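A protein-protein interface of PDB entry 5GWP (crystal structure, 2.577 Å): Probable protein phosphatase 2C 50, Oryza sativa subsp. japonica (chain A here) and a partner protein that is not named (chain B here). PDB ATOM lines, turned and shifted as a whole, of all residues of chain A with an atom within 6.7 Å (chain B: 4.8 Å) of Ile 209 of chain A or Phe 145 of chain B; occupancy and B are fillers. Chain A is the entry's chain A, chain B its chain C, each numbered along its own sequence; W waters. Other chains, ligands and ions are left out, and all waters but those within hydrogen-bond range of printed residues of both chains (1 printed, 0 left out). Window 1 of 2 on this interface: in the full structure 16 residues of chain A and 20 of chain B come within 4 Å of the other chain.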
ATOM      1  N   LYS A 197      -5.675 -21.278  -1.135  1.00  0.00           N
ATOM      2  CA  LYS A 197      -6.294 -20.924   0.133  1.00  0.00           C
ATOM      3  C   LYS A 197      -5.918 -21.940   1.200  1.00  0.00           C
ATOM      4  O   LYS A 197      -5.838 -23.141   0.929  1.00  0.00           O
ATOM      5  CB  LYS A 197      -7.823 -20.853   0.015  1.00  0.00           C
ATOM      6  CG  LYS A 197      -8.341 -19.703  -0.829  1.00  0.00           C
ATOM      7  CD  LYS A 197      -9.852 -19.588  -0.714  1.00  0.00           C
ATOM      8  CE  LYS A 197     -10.403 -18.525  -1.649  1.00  0.00           C
ATOM      9  NZ  LYS A 197     -11.880 -18.383  -1.512  1.00  0.00           N
ATOM     10  N   ILE A 199      -7.618 -23.078   4.591  1.00  0.00           N
ATOM     11  CA  ILE A 199      -8.922 -22.956   5.231  1.00  0.00           C
ATOM     12  C   ILE A 199      -8.948 -23.806   6.493  1.00  0.00           C
ATOM     13  O   ILE A 199      -8.491 -24.955   6.492  1.00  0.00           O
ATOM     14  CB  ILE A 199     -10.061 -23.365   4.274  1.00  0.00           C
ATOM     15  CG1 ILE A 199     -10.006 -22.534   2.991  1.00  0.00           C
ATOM     16  CG2 ILE A 199     -11.416 -23.202   4.946  1.00  0.00           C
ATOM     17  CD1 ILE A 199     -10.950 -23.024   1.911  1.00  0.00           C
ATOM     18  N   TRP A 201     -10.789 -26.104   8.381  1.00  0.00           N
ATOM     19  CA  TRP A 201     -11.900 -27.022   8.112  1.00  0.00           C
ATOM     20  C   TRP A 201     -11.544 -28.349   8.780  1.00  0.00           C
ATOM     21  O   TRP A 201     -10.966 -29.235   8.144  1.00  0.00           O
ATOM     22  CB  TRP A 201     -12.138 -27.181   6.617  1.00  0.00           C
ATOM     23  CG  TRP A 201     -13.512 -27.660   6.275  1.00  0.00           C
ATOM     24  CD1 TRP A 201     -13.992 -28.931   6.394  1.00  0.00           C
ATOM     25  CD2 TRP A 201     -14.587 -26.871   5.755  1.00  0.00           C
ATOM     26  NE1 TRP A 201     -15.302 -28.982   5.981  1.00  0.00           N
ATOM     27  CE2 TRP A 201     -15.691 -27.730   5.583  1.00  0.00           C
ATOM     28  CE3 TRP A 201     -14.725 -25.521   5.417  1.00  0.00           C
ATOM     29  CZ2 TRP A 201     -16.915 -27.283   5.091  1.00  0.00           C
ATOM     30  CZ3 TRP A 201     -15.940 -25.080   4.927  1.00  0.00           C
ATOM     31  CH2 TRP A 201     -17.019 -25.958   4.767  1.00  0.00           C
ATOM     32  N   ARG A 205      -6.081 -26.578   6.472  1.00  0.00           N
ATOM     33  CA  ARG A 205      -5.875 -27.463   5.336  1.00  0.00           C
ATOM     34  C   ARG A 205      -5.710 -26.658   4.054  1.00  0.00           C
ATOM     35  O   ARG A 205      -6.294 -25.582   3.894  1.00  0.00           O
ATOM     36  CB  ARG A 205      -7.045 -28.448   5.182  1.00  0.00           C
ATOM     37  CG  ARG A 205      -7.261 -29.356   6.383  1.00  0.00           C
ATOM     38  CD  ARG A 205      -8.481 -30.246   6.216  1.00  0.00           C
ATOM     39  NE  ARG A 205      -8.719 -31.046   7.413  1.00  0.00           N
ATOM     40  CZ  ARG A 205      -8.345 -32.314   7.550  1.00  0.00           C
ATOM     41  NH1 ARG A 205      -7.714 -32.931   6.561  1.00  0.00           N
ATOM     42  NH2 ARG A 205      -8.597 -32.964   8.678  1.00  0.00           N
ATOM     43  N   VAL A 206      -4.900 -27.194   3.142  1.00  0.00           N
ATOM     44  CA  VAL A 206      -4.800 -26.640   1.795  1.00  0.00           C
ATOM     45  C   VAL A 206      -6.126 -26.867   1.081  1.00  0.00           C
ATOM     46  O   VAL A 206      -6.592 -28.006   0.958  1.00  0.00           O
ATOM     47  CB  VAL A 206      -3.640 -27.276   1.020  1.00  0.00           C
ATOM     48  CG1 VAL A 206      -3.602 -26.745  -0.406  1.00  0.00           C
ATOM     49  CG2 VAL A 206      -2.320 -27.016   1.726  1.00  0.00           C
ATOM     50  N   SER A 207      -6.742 -25.780   0.611  1.00  0.00           N
ATOM     51  CA  SER A 207      -8.067 -25.806  -0.011  1.00  0.00           C
ATOM     52  C   SER A 207      -9.121 -26.428   0.900  1.00  0.00           C
ATOM     53  O   SER A 207     -10.168 -26.880   0.426  1.00  0.00           O
ATOM     54  CB  SER A 207      -8.043 -26.541  -1.358  1.00  0.00           C
ATOM     55  OG  SER A 207      -7.033 -26.029  -2.208  1.00  0.00           O
ATOM     56  N   GLY A 208      -8.860 -26.467   2.205  1.00  0.00           N
ATOM     57  CA  GLY A 208      -9.746 -27.130   3.137  1.00  0.00           C
ATOM     58  C   GLY A 208      -9.733 -28.639   3.077  1.00  0.00           C
ATOM     59  O   GLY A 208     -10.543 -29.276   3.755  1.00  0.00           O
ATOM     60  N   ILE A 209      -8.829 -29.240   2.303  1.00  0.00           N
ATOM     61  CA  ILE A 209      -8.813 -30.684   2.078  1.00  0.00           C
ATOM     62  C   ILE A 209      -7.650 -31.354   2.806  1.00  0.00           C
ATOM     63  O   ILE A 209      -7.857 -32.172   3.704  1.00  0.00           O
ATOM     64  CB  ILE A 209      -8.788 -31.009   0.568  1.00  0.00           C
ATOM     65  CG1 ILE A 209     -10.020 -30.420  -0.123  1.00  0.00           C
ATOM     66  CG2 ILE A 209      -8.722 -32.512   0.353  1.00  0.00           C
ATOM     67  CD1 ILE A 209     -10.007 -30.570  -1.630  1.00  0.00           C
ATOM     68  N   LEU A 210      -6.417 -31.017   2.437  1.00  0.00           N
ATOM     69  CA  LEU A 210      -5.238 -31.741   2.893  1.00  0.00           C
ATOM     70  C   LEU A 210      -4.587 -31.004   4.054  1.00  0.00           C
ATOM     71  O   LEU A 210      -4.299 -29.808   3.954  1.00  0.00           O
ATOM     72  CB  LEU A 210      -4.238 -31.912   1.750  1.00  0.00           C
ATOM     73  CG  LEU A 210      -3.088 -32.893   1.971  1.00  0.00           C
ATOM     74  CD1 LEU A 210      -3.615 -34.315   2.057  1.00  0.00           C
ATOM     75  CD2 LEU A 210      -2.062 -32.762   0.859  1.00  0.00           C
ATOM     76  N   ALA A 211      -4.332 -31.731   5.144  1.00  0.00           N
ATOM     77  CA  ALA A 211      -3.812 -31.156   6.378  1.00  0.00           C
ATOM     78  C   ALA A 211      -2.301 -30.958   6.361  1.00  0.00           C
ATOM     79  O   ALA A 211      -1.698 -30.828   7.433  1.00  0.00           O
ATOM     80  CB  ALA A 211      -4.208 -32.026   7.573  1.00  0.00           C
ATOM     81  N   MET A 212      -1.675 -30.932   5.186  1.00  0.00           N
ATOM     82  CA  MET A 212      -0.258 -30.620   5.088  1.00  0.00           C
ATOM     83  C   MET A 212      -0.018 -29.835   3.808  1.00  0.00           C
ATOM     84  O   MET A 212      -0.795 -29.922   2.853  1.00  0.00           O
ATOM     85  CB  MET A 212       0.615 -31.882   5.115  1.00  0.00           C
ATOM     86  CG  MET A 212       0.567 -32.705   3.841  1.00  0.00           C
ATOM     87  SD  MET A 212       1.205 -34.374   4.077  1.00  0.00           S
ATOM     88  CE  MET A 212       0.050 -35.005   5.291  1.00  0.00           C
ATOM     89  N   TYR A 220      -3.254 -33.308  -7.727  1.00  0.00           N
ATOM     90  CA  TYR A 220      -4.485 -32.534  -7.828  1.00  0.00           C
ATOM     91  C   TYR A 220      -4.454 -31.262  -6.992  1.00  0.00           C
ATOM     92  O   TYR A 220      -5.308 -30.394  -7.193  1.00  0.00           O
ATOM     93  CB  TYR A 220      -5.685 -33.390  -7.413  1.00  0.00           C
ATOM     94  CG  TYR A 220      -5.924 -33.464  -5.920  1.00  0.00           C
ATOM     95  CD1 TYR A 220      -5.042 -34.139  -5.087  1.00  0.00           C
ATOM     96  CD2 TYR A 220      -7.045 -32.875  -5.348  1.00  0.00           C
ATOM     97  CE1 TYR A 220      -5.262 -34.216  -3.724  1.00  0.00           C
ATOM     98  CE2 TYR A 220      -7.274 -32.947  -3.986  1.00  0.00           C
ATOM     99  CZ  TYR A 220      -6.380 -33.619  -3.180  1.00  0.00           C
ATOM    100  OH  TYR A 220      -6.601 -33.693  -1.825  1.00  0.00           O
ATOM    101  N   LEU A 221      -3.499 -31.126  -6.071  1.00  0.00           N
ATOM    102  CA  LEU A 221      -3.373 -29.935  -5.243  1.00  0.00           C
ATOM    103  C   LEU A 221      -2.140 -29.107  -5.583  1.00  0.00           C
ATOM    104  O   LEU A 221      -1.753 -28.236  -4.798  1.00  0.00           O
ATOM    105  CB  LEU A 221      -3.354 -30.321  -3.762  1.00  0.00           C
ATOM    106  CG  LEU A 221      -4.725 -30.540  -3.122  1.00  0.00           C
ATOM    107  CD1 LEU A 221      -4.579 -31.003  -1.685  1.00  0.00           C
ATOM    108  CD2 LEU A 221      -5.560 -29.269  -3.196  1.00  0.00           C
ATOM    109  N   PHE B  49     -12.448 -39.976  -3.712  1.00  0.00           N
ATOM    110  CA  PHE B  49     -12.363 -39.974  -2.261  1.00  0.00           C
ATOM    111  C   PHE B  49     -13.221 -41.044  -1.606  1.00  0.00           C
ATOM    112  O   PHE B  49     -13.096 -41.255  -0.397  1.00  0.00           O
ATOM    113  CB  PHE B  49     -12.749 -38.598  -1.706  1.00  0.00           C
ATOM    114  CG  PHE B  49     -11.909 -37.474  -2.238  1.00  0.00           C
ATOM    115  CD1 PHE B  49     -10.623 -37.272  -1.765  1.00  0.00           C
ATOM    116  CD2 PHE B  49     -12.405 -36.614  -3.204  1.00  0.00           C
ATOM    117  CE1 PHE B  49      -9.845 -36.240  -2.251  1.00  0.00           C
ATOM    118  CE2 PHE B  49     -11.632 -35.579  -3.692  1.00  0.00           C
ATOM    119  CZ  PHE B  49     -10.350 -35.393  -3.215  1.00  0.00           C
ATOM    120  N   GLY B  72      -6.915 -38.624   4.712  1.00  0.00           N
ATOM    121  CA  GLY B  72      -6.452 -37.327   4.263  1.00  0.00           C
ATOM    122  C   GLY B  72      -7.544 -36.312   4.023  1.00  0.00           C
ATOM    123  O   GLY B  72      -7.325 -35.346   3.286  1.00  0.00           O
ATOM    124  N   LEU B  73      -8.717 -36.501   4.616  1.00  0.00           N
ATOM    125  CA  LEU B  73      -9.879 -35.661   4.389  1.00  0.00           C
ATOM    126  C   LEU B  73     -10.406 -35.106   5.707  1.00  0.00           C
ATOM    127  O   LEU B  73     -10.121 -35.652   6.779  1.00  0.00           O
ATOM    128  CB  LEU B  73     -10.979 -36.462   3.677  1.00  0.00           C
ATOM    129  CG  LEU B  73     -10.678 -36.790   2.212  1.00  0.00           C
ATOM    130  CD1 LEU B  73     -11.687 -37.784   1.661  1.00  0.00           C
ATOM    131  CD2 LEU B  73     -10.659 -35.520   1.375  1.00  0.00           C
ATOM    132  N   PRO B  74     -11.179 -34.012   5.665  1.00  0.00           N
ATOM    133  CA  PRO B  74     -11.732 -33.450   6.907  1.00  0.00           C
ATOM    134  C   PRO B  74     -12.842 -34.281   7.528  1.00  0.00           C
ATOM    135  O   PRO B  74     -13.309 -33.935   8.620  1.00  0.00           O
ATOM    136  CB  PRO B  74     -12.271 -32.077   6.467  1.00  0.00           C
ATOM    137  CG  PRO B  74     -11.707 -31.831   5.112  1.00  0.00           C
ATOM    138  CD  PRO B  74     -11.469 -33.164   4.499  1.00  0.00           C
ATOM    139  N   LEU B 103     -20.772 -30.034   6.196  1.00  0.00           N
ATOM    140  CA  LEU B 103     -21.567 -29.598   5.049  1.00  0.00           C
ATOM    141  C   LEU B 103     -23.041 -29.789   5.398  1.00  0.00           C
ATOM    142  O   LEU B 103     -23.684 -30.754   4.984  1.00  0.00           O
ATOM    143  CB  LEU B 103     -21.174 -30.371   3.789  1.00  0.00           C
ATOM    144  CG  LEU B 103     -19.739 -30.153   3.307  1.00  0.00           C
ATOM    145  CD1 LEU B 103     -19.473 -30.957   2.045  1.00  0.00           C
ATOM    146  CD2 LEU B 103     -19.477 -28.674   3.068  1.00  0.00           C
ATOM    147  N   GLU B 141     -14.622 -19.448   1.400  1.00  0.00           N
ATOM    148  CA  GLU B 141     -13.939 -20.657   1.849  1.00  0.00           C
ATOM    149  C   GLU B 141     -14.787 -21.898   1.596  1.00  0.00           C
ATOM    150  O   GLU B 141     -14.295 -22.901   1.063  1.00  0.00           O
ATOM    151  CB  GLU B 141     -13.581 -20.539   3.329  1.00  0.00           C
ATOM    152  CG  GLU B 141     -12.369 -19.665   3.602  1.00  0.00           C
ATOM    153  CD  GLU B 141     -12.116 -19.470   5.085  1.00  0.00           C
ATOM    154  OE1 GLU B 141     -13.080 -19.590   5.872  1.00  0.00           O
ATOM    155  OE2 GLU B 141     -10.956 -19.204   5.465  1.00  0.00           O
ATOM    156  N   THR B 142     -16.069 -21.847   1.968  1.00  0.00           N
ATOM    157  CA  THR B 142     -16.946 -23.000   1.778  1.00  0.00           C
ATOM    158  C   THR B 142     -17.074 -23.346   0.298  1.00  0.00           C
ATOM    159  O   THR B 142     -16.894 -24.505  -0.104  1.00  0.00           O
ATOM    160  CB  THR B 142     -18.322 -22.719   2.387  1.00  0.00           C
ATOM    161  OG1 THR B 142     -18.171 -22.312   3.752  1.00  0.00           O
ATOM    162  CG2 THR B 142     -19.186 -23.971   2.344  1.00  0.00           C
ATOM    163  N   CYS B 143     -17.376 -22.342  -0.531  1.00  0.00           N
ATOM    164  CA  CYS B 143     -17.489 -22.582  -1.966  1.00  0.00           C
ATOM    165  C   CYS B 143     -16.169 -23.041  -2.568  1.00  0.00           C
ATOM    166  O   CYS B 143     -16.168 -23.845  -3.501  1.00  0.00           O
ATOM    167  CB  CYS B 143     -17.980 -21.321  -2.677  1.00  0.00           C
ATOM    168  SG  CYS B 143     -19.770 -21.256  -2.914  1.00  0.00           S
ATOM    169  N   TYR B 144     -15.040 -22.544  -2.059  1.00  0.00           N
ATOM    170  CA  TYR B 144     -13.748 -22.978  -2.582  1.00  0.00           C
ATOM    171  C   TYR B 144     -13.490 -24.448  -2.265  1.00  0.00           C
ATOM    172  O   TYR B 144     -13.020 -25.205  -3.123  1.00  0.00           O
ATOM    173  CB  TYR B 144     -12.635 -22.098  -2.015  1.00  0.00           C
ATOM    174  CG  TYR B 144     -11.305 -22.271  -2.708  1.00  0.00           C
ATOM    175  CD1 TYR B 144     -10.978 -21.501  -3.816  1.00  0.00           C
ATOM    176  CD2 TYR B 144     -10.375 -23.199  -2.257  1.00  0.00           C
ATOM    177  CE1 TYR B 144      -9.767 -21.648  -4.459  1.00  0.00           C
ATOM    178  CE2 TYR B 144      -9.158 -23.354  -2.894  1.00  0.00           C
ATOM    179  CZ  TYR B 144      -8.860 -22.575  -3.995  1.00  0.00           C
ATOM    180  OH  TYR B 144      -7.651 -22.724  -4.633  1.00  0.00           O
ATOM    181  N   PHE B 145     -13.790 -24.862  -1.032  1.00  0.00           N
ATOM    182  CA  PHE B 145     -13.591 -26.250  -0.627  1.00  0.00           C
ATOM    183  C   PHE B 145     -14.486 -27.189  -1.432  1.00  0.00           C
ATOM    184  O   PHE B 145     -14.018 -28.186  -2.006  1.00  0.00           O
ATOM    185  CB  PHE B 145     -13.858 -26.352   0.880  1.00  0.00           C
ATOM    186  CG  PHE B 145     -14.062 -27.747   1.396  1.00  0.00           C
ATOM    187  CD1 PHE B 145     -12.979 -28.567   1.666  1.00  0.00           C
ATOM    188  CD2 PHE B 145     -15.336 -28.212   1.678  1.00  0.00           C
ATOM    189  CE1 PHE B 145     -13.169 -29.843   2.169  1.00  0.00           C
ATOM    190  CE2 PHE B 145     -15.531 -29.486   2.181  1.00  0.00           C
ATOM    191  CZ  PHE B 145     -14.446 -30.300   2.428  1.00  0.00           C
ATOM    192  N   VAL B 146     -15.774 -26.846  -1.538  1.00  0.00           N
ATOM    193  CA  VAL B 146     -16.700 -27.700  -2.274  1.00  0.00           C
ATOM    194  C   VAL B 146     -16.339 -27.727  -3.754  1.00  0.00           C
ATOM    195  O   VAL B 146     -16.377 -28.784  -4.394  1.00  0.00           O
ATOM    196  CB  VAL B 146     -18.151 -27.236  -2.049  1.00  0.00           C
ATOM    197  CG1 VAL B 146     -19.114 -28.093  -2.860  1.00  0.00           C
ATOM    198  CG2 VAL B 146     -18.501 -27.290  -0.569  1.00  0.00           C
ATOM    199  N   GLU B 147     -15.964 -26.575  -4.320  1.00  0.00           N
ATOM    200  CA  GLU B 147     -15.541 -26.544  -5.718  1.00  0.00           C
ATOM    201  C   GLU B 147     -14.298 -27.389  -5.946  1.00  0.00           C
ATOM    202  O   GLU B 147     -14.151 -28.006  -7.003  1.00  0.00           O
ATOM    203  CB  GLU B 147     -15.295 -25.104  -6.174  1.00  0.00           C
ATOM    204  CG  GLU B 147     -16.550 -24.288  -6.438  1.00  0.00           C
ATOM    205  CD  GLU B 147     -16.236 -22.836  -6.750  1.00  0.00           C
ATOM    206  OE1 GLU B 147     -17.145 -22.112  -7.208  1.00  0.00           O
ATOM    207  OE2 GLU B 147     -15.077 -22.420  -6.539  1.00  0.00           O
ATOM    208  N   ALA B 148     -13.383 -27.422  -4.977  1.00  0.00           N
ATOM    209  CA  ALA B 148     -12.199 -28.258  -5.136  1.00  0.00           C
ATOM    210  C   ALA B 148     -12.576 -29.735  -5.179  1.00  0.00           C
ATOM    211  O   ALA B 148     -12.147 -30.474  -6.080  1.00  0.00           O
ATOM    212  CB  ALA B 148     -11.203 -27.987  -4.010  1.00  0.00           C
ATOM    213  N   LEU B 149     -13.410 -30.178  -4.231  1.00  0.00           N
ATOM    214  CA  LEU B 149     -13.824 -31.580  -4.242  1.00  0.00           C
ATOM    215  C   LEU B 149     -14.586 -31.925  -5.519  1.00  0.00           C
ATOM    216  O   LEU B 149     -14.354 -32.978  -6.128  1.00  0.00           O
ATOM    217  CB  LEU B 149     -14.673 -31.889  -3.011  1.00  0.00           C
ATOM    218  CG  LEU B 149     -13.955 -31.825  -1.665  1.00  0.00           C
ATOM    219  CD1 LEU B 149     -14.963 -31.952  -0.539  1.00  0.00           C
ATOM    220  CD2 LEU B 149     -12.897 -32.913  -1.572  1.00  0.00           C
HETATM  221  O   HOH W   1      -5.682 -23.945  -2.322  1.00  0.00           O
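Water W1 lies within hydrogen-bond range of OG of Ser 207 of chain A (2.5 Å), N of Lys 197 of chain A (2.9 Å) and OH of Tyr 144 of chain B (3.3 Å).
Among the printed residues, merely in contact across the chains: Lys 197 of chain A with Tyr 144 of chain B (3.6 Å), Ile 199 of chain A with Glu 141 of chain B (3.5 Å), Trp 201 of chain A with Pro 74 of chain B (3.5 Å), Trp 201 of chain A with Leu 103 of chain B (3.5 Å), Trp 201 of chain A with Thr 142 of chain B (3.7 Å), Trp 201 of chain A with Phe 145 of chain B (3.8 Å), Arg 205 of chain A with Leu 73 of chain B (3.6 Å), Arg 205 of chain A with Pro 74 of chain B (3.6 Å), Ser 207 of chain A with Tyr 144 of chain B (3.5 Å), Ser 207 of chain A with Phe 145 of chain B (3.5 Å), Gly 208 of chain A with Pro 74 of chain B (3.1 Å), Gly 208 of chain A with Phe 145 of chain B (3.1 Å), Ile 209 of chain A with Leu 73 of chain B (3.7 Å), Ile 209 of chain A with Pro 74 of chain B (3.8 Å), Ile 209 of chain A with Phe 145 of chain B (3.9 Å), Ile 209 of chain A with Ala 148 of chain B (3.7 Å) and Ile 209 of chain A with Leu 149 of chain B (3.7 Å).
Hydrophobic or aromatic side chains of chain B that line the printed part of chain A: Leu 73, Pro 74, Leu 103, Tyr 144, Phe 145, Ala 148 and Leu 149.
Printed residues of chain A that touch a printed residue of chain B: Lys 197, Ile 199, Trp 201, Arg 205, Ser 207, Gly 208 and Ile 209.
Among the printed residues, no Asp or Glu carboxylate lies within 4 Å of a Lys or Arg side-chain nitrogen of the other chain.
The backbone carbonyl oxygen (O) of Lys 197 of chain A sits at hydrogen-bond distance from the backbone NH (N) of Ser 207 of chain A, at 2.8 Å.
NH1 of Arg 205 of chain A sits at hydrogen-bond distance from O of Ile 209 of chain A, at 3.0 Å.
The backbone NH (N) of Arg 205 of chain A is in hydrogen-bond range of the backbone carbonyl oxygen (O) of Ile 199 of chain A.
NE of Arg 205 of chain A lies within hydrogen-bond range of O of Trp 201 of chain A (3.0 Å).
Ile 209 of chain A touches just these residues of chain B: Gly 72 (3.2 Å), Leu 73 (3.7 Å), Pro 74 (3.8 Å), Phe 145 (3.9 Å), Ala 148 (3.7 Å) and Leu 149 (3.7 Å).
Phe 145 of chain B touches just these residues of chain A: Trp 201 (3.8 Å), Ser 207 (3.5 Å), Gly 208 (3.1 Å) and Ile 209 (3.9 Å).
Printed residues of chain B within 4 Å of Trp 201 of chain A: Pro 74 (3.5 Å), Leu 103 (3.5 Å), Thr 142 (3.7 Å) and Phe 145 (3.8 Å).
Printed residues of chain B within 4 Å of Ser 207 of chain A: Tyr 144 (3.5 Å) and Phe 145 (3.5 Å).
Printed residues of chain B within 4 Å of Gly 208 of chain A: Pro 74 (3.1 Å) and Phe 145 (3.1 Å).
Printed residues of chain A within 4 Å of Thr 142 of chain B: Trp 201 (3.7 Å).
Printed residues of chain A within 4 Å of Gly 72 of chain B: Ile 209 (3.2 Å).
The nearest printed residue of chain A that does not touch Glu 141 of chain B is Lys 197 of chain A (4.1 Å).
O of Ile 209 of chain A sits close to O of Gly 72 of chain B.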
